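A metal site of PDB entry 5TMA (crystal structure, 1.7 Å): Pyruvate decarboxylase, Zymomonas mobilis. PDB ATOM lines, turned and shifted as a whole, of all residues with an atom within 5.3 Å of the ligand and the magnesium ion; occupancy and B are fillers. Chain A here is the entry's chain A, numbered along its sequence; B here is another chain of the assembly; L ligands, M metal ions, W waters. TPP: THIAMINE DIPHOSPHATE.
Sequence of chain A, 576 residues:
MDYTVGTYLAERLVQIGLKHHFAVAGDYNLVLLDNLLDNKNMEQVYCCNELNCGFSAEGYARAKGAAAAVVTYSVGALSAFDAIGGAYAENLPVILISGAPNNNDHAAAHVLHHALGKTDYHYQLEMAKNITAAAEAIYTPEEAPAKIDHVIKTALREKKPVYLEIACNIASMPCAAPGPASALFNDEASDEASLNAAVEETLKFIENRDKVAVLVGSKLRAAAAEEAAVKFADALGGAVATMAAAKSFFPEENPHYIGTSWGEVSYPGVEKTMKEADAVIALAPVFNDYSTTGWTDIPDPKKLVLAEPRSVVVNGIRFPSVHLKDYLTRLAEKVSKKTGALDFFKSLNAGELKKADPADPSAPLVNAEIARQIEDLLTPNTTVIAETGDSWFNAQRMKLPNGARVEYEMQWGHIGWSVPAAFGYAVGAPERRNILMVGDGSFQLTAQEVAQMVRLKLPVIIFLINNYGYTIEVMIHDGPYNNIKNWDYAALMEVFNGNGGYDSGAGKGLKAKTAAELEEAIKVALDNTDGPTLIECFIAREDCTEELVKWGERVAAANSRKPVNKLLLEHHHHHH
N of Gly 441 sits close to O1A of the ligand (2.9 Å).
N of Thr 471 sits at hydrogen-bond distance from O1B of the ligand (3.2 Å).
O3B of the ligand sits at hydrogen-bond distance from N of Asp 390 (2.8 Å).
OG of Ser 442 lies within hydrogen-bond range of O2A of the ligand (2.5 Å).
N of Ser 442 lies within hydrogen-bond range of O2A of the ligand (2.8 Å).
O1B of the ligand is in hydrogen-bond range of N of Ile 472 (2.7 Å).
The backbone NH (N) of Ile 415 sits at hydrogen-bond distance from a nitrogen (N3') of the ligand, at 3.0 Å.
OE2 of Glu 50 of chain B lies within hydrogen-bond range of N1' of the ligand, 2.5 Å away.
The backbone carbonyl oxygen (O) of Gly 413 sits at hydrogen-bond distance from a nitrogen (N4') of the ligand, at 2.6 Å.
The side-chain hydroxyl (OG1) of Thr 471 sits at hydrogen-bond distance from the side-chain amide nitrogen (ND2) of Asn 467 (3.1 Å).
The side-chain carboxylate (OE1) of Glu 473 lies within hydrogen-bond range of the backbone NH (N) of Asp 27 of chain B, 3.4 Å away.
The backbone NH (N) of Asp 440 sits at hydrogen-bond distance from the backbone carbonyl oxygen (O) of Ile 465, 3.1 Å away.
OG of Ser 442 is in hydrogen-bond range of O of Thr 388.
OD2 of Asp 440 lies within hydrogen-bond range of N of Tyr 468, 3.0 Å away.
Merely in contact with the ligand: His 114 of chain B (3.3 Å), Ala 25 of chain B (3.3 Å), His 414 (3.3 Å), Tyr 470 (3.3 Å), Val 75 of chain B (3.4 Å), Gly 26 of chain B (3.5 Å), Glu 473 (3.6 Å), Gly 439 (3.6 Å), Gly 389 (3.7 Å), Thr 388 (3.8 Å), Leu 445 (3.9 Å) and Thr 72 of chain B (3.98 Å).
Hydrophobic or aromatic side chains within 4 Å of the ligand: His 414, Ile 415, Leu 445, Tyr 470, Ile 472, Val 75 of chain B and His 114 of chain B.
Of the 31 residues printed, 23 come within 4 Å of the ligand.
Three residues have an atom within 4 Å of the magnesium ion: Asp 440, Asn 467 and Gly 469.
O1A of the ligand binds the magnesium ion (2.0 Å).
An oxygen (O2B) of the ligand is bound to the magnesium ion (2.0 Å).
The magnesium ion is bound by O of Gly 469 (2.1 Å).
OD1 of Asp 440 is bound to the magnesium ion (2.1 Å).
Water W4 is bound to the magnesium ion (2.2 Å).
The magnesium ion is bound by OD1 of Asn 467.
Water W4 lies within hydrogen-bond range of O of Ile 465 (2.8 Å), ND2 of Asn 467 (3.2 Å) and N of Asp 440 (3.4 Å).
Water W3 lies within hydrogen-bond range of an oxygen (O2A) of the ligand (2.6 Å), the backbone carbonyl oxygen of Thr 388 (2.9 Å), the backbone NH of Gly 439 (2.9 Å) and the side-chain hydroxyl of Ser 442 (3.2 Å).
Water W1 lies within hydrogen-bond range of the side-chain carboxylate of Glu 473 (2.7 Å) and the backbone NH of Asp 27 of chain B (3.2 Å).
Water W2 lies within hydrogen-bond range of the side-chain hydroxyl of Ser 391 (2.7 Å), an oxygen (O3B) of the ligand (3.3 Å) and the backbone NH of Asp 390 (3.5 Å).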
ATOM      1  N   GLU A 387      20.728  -2.973   9.203  1.00  0.00           N
ATOM      2  CA  GLU A 387      19.460  -2.812   9.932  1.00  0.00           C
ATOM      3  C   GLU A 387      18.900  -1.393   9.822  1.00  0.00           C
ATOM      4  O   GLU A 387      19.664  -0.413   9.648  1.00  0.00           O
ATOM      5  CB  GLU A 387      19.716  -3.145  11.380  1.00  0.00           C
ATOM      6  CG  GLU A 387      18.505  -3.272  12.303  1.00  0.00           C
ATOM      7  CD  GLU A 387      17.513  -4.275  11.809  1.00  0.00           C
ATOM      8  OE1 GLU A 387      16.710  -3.939  10.908  1.00  0.00           O
ATOM      9  OE2 GLU A 387      17.477  -5.385  12.303  1.00  0.00           O
ATOM     10  N   THR A 388      17.554  -1.336   9.981  1.00  0.00           N
ATOM     11  CA  THR A 388      16.809  -0.085  10.243  1.00  0.00           C
ATOM     12  C   THR A 388      17.318   0.572  11.475  1.00  0.00           C
ATOM     13  O   THR A 388      17.436  -0.056  12.504  1.00  0.00           O
ATOM     14  CB  THR A 388      15.297  -0.368  10.386  1.00  0.00           C
ATOM     15  OG1 THR A 388      14.819  -0.856   9.112  1.00  0.00           O
ATOM     16  CG2 THR A 388      14.611   0.848  10.737  1.00  0.00           C
ATOM     17  N   GLY A 389      17.687   1.825  11.344  1.00  0.00           N
ATOM     18  CA  GLY A 389      18.402   2.513  12.430  1.00  0.00           C
ATOM     19  C   GLY A 389      19.399   3.439  11.784  1.00  0.00           C
ATOM     20  O   GLY A 389      19.413   3.602  10.537  1.00  0.00           O
ATOM     21  N   ASP A 390      20.281   4.042  12.575  1.00  0.00           N
ATOM     22  CA  ASP A 390      21.380   4.811  11.923  1.00  0.00           C
ATOM     23  C   ASP A 390      22.238   3.977  10.943  1.00  0.00           C
ATOM     24  O   ASP A 390      22.822   4.571  10.038  1.00  0.00           O
ATOM     25  CB  ASP A 390      22.307   5.518  12.943  1.00  0.00           C
ATOM     26  CG  ASP A 390      22.932   6.804  12.379  1.00  0.00           C
ATOM     27  OD1 ASP A 390      22.373   7.387  11.402  1.00  0.00           O
ATOM     28  OD2 ASP A 390      24.009   7.221  12.887  1.00  0.00           O
ATOM     29  N   SER A 391      22.298   2.618  11.091  1.00  0.00           N
ATOM     30  CA  SER A 391      23.010   1.782  10.194  1.00  0.00           C
ATOM     31  C   SER A 391      22.533   1.958   8.757  1.00  0.00           C
ATOM     32  O   SER A 391      23.321   1.738   7.864  1.00  0.00           O
ATOM     33  CB  SER A 391      22.883   0.288  10.603  1.00  0.00           C
ATOM     34  OG  SER A 391      23.615  -0.009  11.828  1.00  0.00           O
ATOM     35  N   GLY A 413      10.827  -2.453   7.087  1.00  0.00           N
ATOM     36  CA  GLY A 413      11.437  -1.721   8.248  1.00  0.00           C
ATOM     37  C   GLY A 413      11.170  -2.302   9.617  1.00  0.00           C
ATOM     38  O   GLY A 413      10.877  -1.571  10.533  1.00  0.00           O
ATOM     39  N   HIS A 414      11.239  -3.632   9.754  1.00  0.00           N
ATOM     40  CA  HIS A 414      10.977  -4.302  11.028  1.00  0.00           C
ATOM     41  C   HIS A 414      12.284  -4.374  11.777  1.00  0.00           C
ATOM     42  O   HIS A 414      13.147  -5.149  11.372  1.00  0.00           O
ATOM     43  CB  HIS A 414      10.430  -5.697  10.753  1.00  0.00           C
ATOM     44  CG  HIS A 414      10.006  -6.427  11.957  1.00  0.00           C
ATOM     45  ND1 HIS A 414      10.876  -6.739  12.977  1.00  0.00           N
ATOM     46  CD2 HIS A 414       8.835  -7.014  12.282  1.00  0.00           C
ATOM     47  CE1 HIS A 414      10.224  -7.409  13.915  1.00  0.00           C
ATOM     48  NE2 HIS A 414       8.997  -7.599  13.508  1.00  0.00           N
ATOM     49  N   ILE A 415      12.429  -3.612  12.865  1.00  0.00           N
ATOM     50  CA  ILE A 415      13.703  -3.661  13.551  1.00  0.00           C
ATOM     51  C   ILE A 415      13.887  -5.055  14.091  1.00  0.00           C
ATOM     52  O   ILE A 415      12.943  -5.739  14.498  1.00  0.00           O
ATOM     53  CB  ILE A 415      13.849  -2.578  14.609  1.00  0.00           C
ATOM     54  CG1 ILE A 415      12.777  -2.626  15.678  1.00  0.00           C
ATOM     55  CG2 ILE A 415      13.994  -1.231  13.894  1.00  0.00           C
ATOM     56  CD1 ILE A 415      13.213  -1.935  16.988  1.00  0.00           C
ATOM     57  N   GLY A 439      21.960  -2.162  15.278  1.00  0.00           N
ATOM     58  CA  GLY A 439      21.861  -1.398  16.511  1.00  0.00           C
ATOM     59  C   GLY A 439      21.404  -2.236  17.688  1.00  0.00           C
ATOM     60  O   GLY A 439      20.750  -3.286  17.540  1.00  0.00           O
ATOM     61  N   ASP A 440      21.721  -1.736  18.874  1.00  0.00           N
ATOM     62  CA  ASP A 440      21.354  -2.411  20.140  1.00  0.00           C
ATOM     63  C   ASP A 440      19.879  -2.666  20.255  1.00  0.00           C
ATOM     64  O   ASP A 440      19.463  -3.780  20.606  1.00  0.00           O
ATOM     65  CB  ASP A 440      21.932  -1.677  21.338  1.00  0.00           C
ATOM     66  CG  ASP A 440      21.451  -0.167  21.429  1.00  0.00           C
ATOM     67  OD1 ASP A 440      21.169   0.501  20.386  1.00  0.00           O
ATOM     68  OD2 ASP A 440      21.313   0.351  22.550  1.00  0.00           O
ATOM     69  N   GLY A 441      19.048  -1.659  19.996  1.00  0.00           N
ATOM     70  CA  GLY A 441      17.587  -1.794  20.051  1.00  0.00           C
ATOM     71  C   GLY A 441      16.973  -2.833  19.188  1.00  0.00           C
ATOM     72  O   GLY A 441      16.177  -3.656  19.650  1.00  0.00           O
ATOM     73  N   SER A 442      17.381  -2.833  17.953  1.00  0.00           N
ATOM     74  CA  SER A 442      17.001  -3.864  16.989  1.00  0.00           C
ATOM     75  C   SER A 442      17.454  -5.231  17.390  1.00  0.00           C
ATOM     76  O   SER A 442      16.665  -6.185  17.304  1.00  0.00           O
ATOM     77  CB  SER A 442      17.593  -3.542  15.623  1.00  0.00           C
ATOM     78  OG  SER A 442      17.024  -2.307  15.141  1.00  0.00           O
ATOM     79  N   PHE A 443      18.707  -5.325  17.853  1.00  0.00           N
ATOM     80  CA  PHE A 443      19.299  -6.609  18.165  1.00  0.00           C
ATOM     81  C   PHE A 443      18.437  -7.319  19.188  1.00  0.00           C
ATOM     82  O   PHE A 443      18.274  -8.520  19.123  1.00  0.00           O
ATOM     83  CB  PHE A 443      20.735  -6.424  18.690  1.00  0.00           C
ATOM     84  CG  PHE A 443      21.467  -7.683  18.891  1.00  0.00           C
ATOM     85  CD1 PHE A 443      22.007  -8.377  17.872  1.00  0.00           C
ATOM     86  CD2 PHE A 443      21.631  -8.139  20.182  1.00  0.00           C
ATOM     87  CE1 PHE A 443      22.743  -9.539  18.157  1.00  0.00           C
ATOM     88  CE2 PHE A 443      22.338  -9.289  20.474  1.00  0.00           C
ATOM     89  CZ  PHE A 443      22.873 -10.012  19.444  1.00  0.00           C
ATOM     90  N   LEU A 445      15.301  -7.602  19.640  1.00  0.00           N
ATOM     91  CA  LEU A 445      14.061  -8.251  19.191  1.00  0.00           C
ATOM     92  C   LEU A 445      14.231  -9.695  18.739  1.00  0.00           C
ATOM     93  O   LEU A 445      13.283 -10.502  18.826  1.00  0.00           O
ATOM     94  CB  LEU A 445      13.390  -7.448  18.072  1.00  0.00           C
ATOM     95  CG  LEU A 445      12.589  -6.226  18.509  1.00  0.00           C
ATOM     96  CD1 LEU A 445      13.497  -5.017  18.465  1.00  0.00           C
ATOM     97  CD2 LEU A 445      11.411  -6.028  17.562  1.00  0.00           C
ATOM     98  N   ILE A 465      26.053  -1.884  17.342  1.00  0.00           N
ATOM     99  CA  ILE A 465      26.284  -0.451  17.665  1.00  0.00           C
ATOM    100  C   ILE A 465      25.552  -0.132  18.929  1.00  0.00           C
ATOM    101  O   ILE A 465      24.290  -0.007  18.939  1.00  0.00           O
ATOM    102  CB  ILE A 465      25.828   0.460  16.514  1.00  0.00           C
ATOM    103  CG1 ILE A 465      26.373  -0.058  15.192  1.00  0.00           C
ATOM    104  CG2 ILE A 465      26.201   1.904  16.828  1.00  0.00           C
ATOM    105  CD1 ILE A 465      27.827  -0.223  15.088  1.00  0.00           C
ATOM    106  N   ASN A 467      24.591   2.315  21.241  1.00  0.00           N
ATOM    107  CA  ASN A 467      24.307   3.739  21.553  1.00  0.00           C
ATOM    108  C   ASN A 467      23.120   3.890  22.561  1.00  0.00           C
ATOM    109  O   ASN A 467      22.449   4.921  22.606  1.00  0.00           O
ATOM    110  CB  ASN A 467      24.065   4.540  20.239  1.00  0.00           C
ATOM    111  CG  ASN A 467      22.844   4.096  19.495  1.00  0.00           C
ATOM    112  OD1 ASN A 467      22.055   3.301  20.029  1.00  0.00           O
ATOM    113  ND2 ASN A 467      22.623   4.644  18.292  1.00  0.00           N
ATOM    114  N   TYR A 468      22.836   2.850  23.357  1.00  0.00           N
ATOM    115  CA  TYR A 468      21.933   2.941  24.506  1.00  0.00           C
ATOM    116  C   TYR A 468      20.528   3.443  24.140  1.00  0.00           C
ATOM    117  O   TYR A 468      20.019   4.404  24.710  1.00  0.00           O
ATOM    118  CB  TYR A 468      22.562   3.804  25.626  1.00  0.00           C
ATOM    119  CG  TYR A 468      23.946   3.303  26.038  1.00  0.00           C
ATOM    120  CD1 TYR A 468      24.078   2.274  27.000  1.00  0.00           C
ATOM    121  CD2 TYR A 468      25.132   3.814  25.472  1.00  0.00           C
ATOM    122  CE1 TYR A 468      25.315   1.782  27.393  1.00  0.00           C
ATOM    123  CE2 TYR A 468      26.392   3.331  25.870  1.00  0.00           C
ATOM    124  CZ  TYR A 468      26.463   2.306  26.835  1.00  0.00           C
ATOM    125  OH  TYR A 468      27.693   1.824  27.240  1.00  0.00           O
ATOM    126  N   GLY A 469      19.937   2.796  23.141  1.00  0.00           N
ATOM    127  CA  GLY A 469      18.509   2.967  22.799  1.00  0.00           C
ATOM    128  C   GLY A 469      18.190   3.205  21.320  1.00  0.00           C
ATOM    129  O   GLY A 469      19.027   2.922  20.434  1.00  0.00           O
ATOM    130  N   TYR A 470      16.987   3.763  21.065  1.00  0.00           N
ATOM    131  CA  TYR A 470      16.476   3.840  19.684  1.00  0.00           C
ATOM    132  C   TYR A 470      16.785   5.246  19.099  1.00  0.00           C
ATOM    133  O   TYR A 470      15.921   6.168  19.131  1.00  0.00           O
ATOM    134  CB  TYR A 470      14.946   3.691  19.661  1.00  0.00           C
ATOM    135  CG  TYR A 470      14.389   2.401  20.210  1.00  0.00           C
ATOM    136  CD1 TYR A 470      14.992   1.157  19.999  1.00  0.00           C
ATOM    137  CD2 TYR A 470      13.098   2.407  20.775  1.00  0.00           C
ATOM    138  CE1 TYR A 470      14.384  -0.038  20.430  1.00  0.00           C
ATOM    139  CE2 TYR A 470      12.505   1.250  21.265  1.00  0.00           C
ATOM    140  CZ  TYR A 470      13.139   0.023  21.099  1.00  0.00           C
ATOM    141  OH  TYR A 470      12.510  -1.181  21.575  1.00  0.00           O
ATOM    142  N   THR A 471      18.006   5.413  18.637  1.00  0.00           N
ATOM    143  CA  THR A 471      18.470   6.755  18.263  1.00  0.00           C
ATOM    144  C   THR A 471      17.706   7.304  17.063  1.00  0.00           C
ATOM    145  O   THR A 471      17.365   8.478  17.031  1.00  0.00           O
ATOM    146  CB  THR A 471      20.012   6.756  18.145  1.00  0.00           C
ATOM    147  OG1 THR A 471      20.566   6.677  19.486  1.00  0.00           O
ATOM    148  CG2 THR A 471      20.559   8.040  17.413  1.00  0.00           C
ATOM    149  N   ILE A 472      17.443   6.488  16.060  1.00  0.00           N
ATOM    150  CA  ILE A 472      16.544   6.973  14.959  1.00  0.00           C
ATOM    151  C   ILE A 472      15.160   7.557  15.471  1.00  0.00           C
ATOM    152  O   ILE A 472      14.733   8.623  15.025  1.00  0.00           O
ATOM    153  CB  ILE A 472      16.378   5.851  13.915  1.00  0.00           C
ATOM    154  CG1 ILE A 472      15.618   6.281  12.670  1.00  0.00           C
ATOM    155  CG2 ILE A 472      15.691   4.658  14.547  1.00  0.00           C
ATOM    156  CD1 ILE A 472      15.785   5.272  11.527  1.00  0.00           C
ATOM    157  N   GLU A 473      14.518   6.885  16.458  1.00  0.00           N
ATOM    158  CA  GLU A 473      13.245   7.400  17.025  1.00  0.00           C
ATOM    159  C   GLU A 473      13.533   8.691  17.783  1.00  0.00           C
ATOM    160  O   GLU A 473      12.682   9.623  17.781  1.00  0.00           O
ATOM    161  CB  GLU A 473      12.539   6.412  17.985  1.00  0.00           C
ATOM    162  CG  GLU A 473      12.261   5.036  17.438  1.00  0.00           C
ATOM    163  CD  GLU A 473      11.270   5.067  16.312  1.00  0.00           C
ATOM    164  OE1 GLU A 473      10.130   4.768  16.610  1.00  0.00           O
ATOM    165  OE2 GLU A 473      11.623   5.399  15.162  1.00  0.00           O
ATOM    166  N   VAL B  24       5.522  -1.065  22.543  1.00  0.00           N
ATOM    167  CA  VAL B  24       6.758  -0.923  21.780  1.00  0.00           C
ATOM    168  C   VAL B  24       6.544   0.260  20.871  1.00  0.00           C
ATOM    169  O   VAL B  24       5.623   0.300  20.068  1.00  0.00           O
ATOM    170  CB  VAL B  24       7.088  -2.189  20.931  1.00  0.00           C
ATOM    171  CG1 VAL B  24       8.406  -1.982  20.203  1.00  0.00           C
ATOM    172  CG2 VAL B  24       7.121  -3.400  21.816  1.00  0.00           C
ATOM    173  N   ALA B  25       7.444   1.226  20.995  1.00  0.00           N
ATOM    174  CA  ALA B  25       7.411   2.436  20.161  1.00  0.00           C
ATOM    175  C   ALA B  25       7.666   2.229  18.697  1.00  0.00           C
ATOM    176  O   ALA B  25       8.481   1.407  18.269  1.00  0.00           O
ATOM    177  CB  ALA B  25       8.470   3.396  20.639  1.00  0.00           C
ATOM    178  N   GLY B  26       7.040   3.063  17.917  1.00  0.00           N
ATOM    179  CA  GLY B  26       7.346   3.212  16.505  1.00  0.00           C
ATOM    180  C   GLY B  26       6.739   4.491  15.981  1.00  0.00           C
ATOM    181  O   GLY B  26       5.811   5.105  16.600  1.00  0.00           O
ATOM    182  N   ASP B  27       7.240   4.974  14.865  1.00  0.00           N
ATOM    183  CA  ASP B  27       6.795   6.321  14.452  1.00  0.00           C
ATOM    184  C   ASP B  27       5.267   6.536  14.256  1.00  0.00           C
ATOM    185  O   ASP B  27       4.779   7.650  14.602  1.00  0.00           O
ATOM    186  CB  ASP B  27       7.661   6.902  13.342  1.00  0.00           C
ATOM    187  CG  ASP B  27       7.476   6.226  12.050  1.00  0.00           C
ATOM    188  OD1 ASP B  27       6.938   5.096  12.078  1.00  0.00           O
ATOM    189  OD2 ASP B  27       7.861   6.815  10.983  1.00  0.00           O
ATOM    190  N   GLU B  50       7.220  -7.206  19.891  1.00  0.00           N
ATOM    191  CA  GLU B  50       5.791  -7.141  19.905  1.00  0.00           C
ATOM    192  C   GLU B  50       5.072  -8.437  20.223  1.00  0.00           C
ATOM    193  O   GLU B  50       3.993  -8.376  20.857  1.00  0.00           O
ATOM    194  CB  GLU B  50       5.245  -6.553  18.609  1.00  0.00           C
ATOM    195  CG  GLU B  50       5.635  -5.070  18.470  1.00  0.00           C
ATOM    196  CD  GLU B  50       6.988  -4.877  17.765  1.00  0.00           C
ATOM    197  OE1 GLU B  50       7.739  -5.928  17.477  1.00  0.00           O
ATOM    198  OE2 GLU B  50       7.275  -3.616  17.488  1.00  0.00           O
ATOM    199  N   THR B  72       3.181  -0.575  16.882  1.00  0.00           N
ATOM    200  CA  THR B  72       3.214   0.169  15.620  1.00  0.00           C
ATOM    201  C   THR B  72       2.665  -0.647  14.432  1.00  0.00           C
ATOM    202  O   THR B  72       2.637  -1.867  14.379  1.00  0.00           O
ATOM    203  CB  THR B  72       4.598   0.835  15.220  1.00  0.00           C
ATOM    204  OG1 THR B  72       4.331   2.020  14.394  1.00  0.00           O
ATOM    205  CG2 THR B  72       5.554  -0.210  14.509  1.00  0.00           C
ATOM    206  N   VAL B  75       4.433  -3.864  11.082  1.00  0.00           N
ATOM    207  CA  VAL B  75       5.573  -4.565  11.693  1.00  0.00           C
ATOM    208  C   VAL B  75       5.356  -4.922  13.192  1.00  0.00           C
ATOM    209  O   VAL B  75       5.876  -5.884  13.704  1.00  0.00           O
ATOM    210  CB  VAL B  75       6.893  -3.778  11.485  1.00  0.00           C
ATOM    211  CG1 VAL B  75       7.143  -3.664  10.012  1.00  0.00           C
ATOM    212  CG2 VAL B  75       6.838  -2.384  12.105  1.00  0.00           C
ATOM    213  N   GLY B  76       4.641  -4.092  13.936  1.00  0.00           N
ATOM    214  CA  GLY B  76       4.380  -4.444  15.322  1.00  0.00           C
ATOM    215  C   GLY B  76       3.143  -5.295  15.459  1.00  0.00           C
ATOM    216  O   GLY B  76       3.118  -6.259  16.201  1.00  0.00           O
ATOM    217  N   HIS B 114       6.566   0.468   6.452  1.00  0.00           N
ATOM    218  CA  HIS B 114       5.954  -0.585   7.297  1.00  0.00           C
ATOM    219  C   HIS B 114       4.824  -1.366   6.636  1.00  0.00           C
ATOM    220  O   HIS B 114       4.374  -2.380   7.089  1.00  0.00           O
ATOM    221  CB  HIS B 114       5.476  -0.101   8.654  1.00  0.00           C
ATOM    222  CG  HIS B 114       6.548   0.347   9.604  1.00  0.00           C
ATOM    223  ND1 HIS B 114       7.900   0.130   9.419  1.00  0.00           N
ATOM    224  CD2 HIS B 114       6.445   0.921  10.822  1.00  0.00           C
ATOM    225  CE1 HIS B 114       8.581   0.591  10.453  1.00  0.00           C
ATOM    226  NE2 HIS B 114       7.719   1.096  11.310  1.00  0.00           N
HETATM  227  N1' TPP L   1       8.894  -2.341  16.033  1.00  0.00           N
HETATM  228  C2' TPP L   1       9.281  -2.983  14.865  1.00  0.00           C
HETATM  229  CM2 TPP L   1       9.082  -4.424  14.882  1.00  0.00           C
HETATM  230  N3' TPP L   1       9.833  -2.384  13.813  1.00  0.00           N
HETATM  231  C4' TPP L   1      10.043  -1.055  13.872  1.00  0.00           C
HETATM  232  N4' TPP L   1      10.566  -0.445  12.827  1.00  0.00           N
HETATM  233  C5' TPP L   1       9.684  -0.286  15.090  1.00  0.00           C
HETATM  234  C6' TPP L   1       9.102  -1.003  16.134  1.00  0.00           C
HETATM  235  C7' TPP L   1       9.945   1.220  15.153  1.00  0.00           C
HETATM  236  N3  TPP L   1      11.376   1.588  15.041  1.00  0.00           N
HETATM  237  C2  TPP L   1      12.040   2.071  13.920  1.00  0.00           C
HETATM  238  S1  TPP L   1      13.788   2.405  14.097  1.00  0.00           S
HETATM  239  C5  TPP L   1      13.602   1.972  15.801  1.00  0.00           C
HETATM  240  C4  TPP L   1      12.210   1.567  16.150  1.00  0.00           C
HETATM  241  CM4 TPP L   1      11.773   1.135  17.551  1.00  0.00           C
HETATM  242  C6  TPP L   1      14.840   2.053  16.622  1.00  0.00           C
HETATM  243  C7  TPP L   1      15.980   1.090  16.263  1.00  0.00           C
HETATM  244  O7  TPP L   1      16.953   1.273  17.298  1.00  0.00           O
HETATM  245  PA  TPP L   1      18.473   0.715  17.126  1.00  0.00           P
HETATM  246  O1A TPP L   1      19.134   0.750  18.458  1.00  0.00           O
HETATM  247  O2A TPP L   1      18.350  -0.667  16.442  1.00  0.00           O
HETATM  248  O3A TPP L   1      19.147   1.639  15.987  1.00  0.00           O
HETATM  249  PB  TPP L   1      19.613   3.188  16.274  1.00  0.00           P
HETATM  250  O1B TPP L   1      18.371   3.953  15.788  1.00  0.00           O
HETATM  251  O2B TPP L   1      19.914   3.443  17.732  1.00  0.00           O
HETATM  252  O3B TPP L   1      20.678   3.495  15.297  1.00  0.00           O
HETATM  253 MG    MG M   1      20.436   2.082  19.162  1.00  0.00          MG
HETATM  254  O   HOH W   1       9.903   4.436  13.250  1.00  0.00           O
HETATM  255  O   HOH W   2      21.709   1.004  13.459  1.00  0.00           O
HETATM  256  O   HOH W   3      19.671  -0.752  14.149  1.00  0.00           O
HETATM  257  O   HOH W   4      22.105   1.486  17.892  1.00  0.00           O
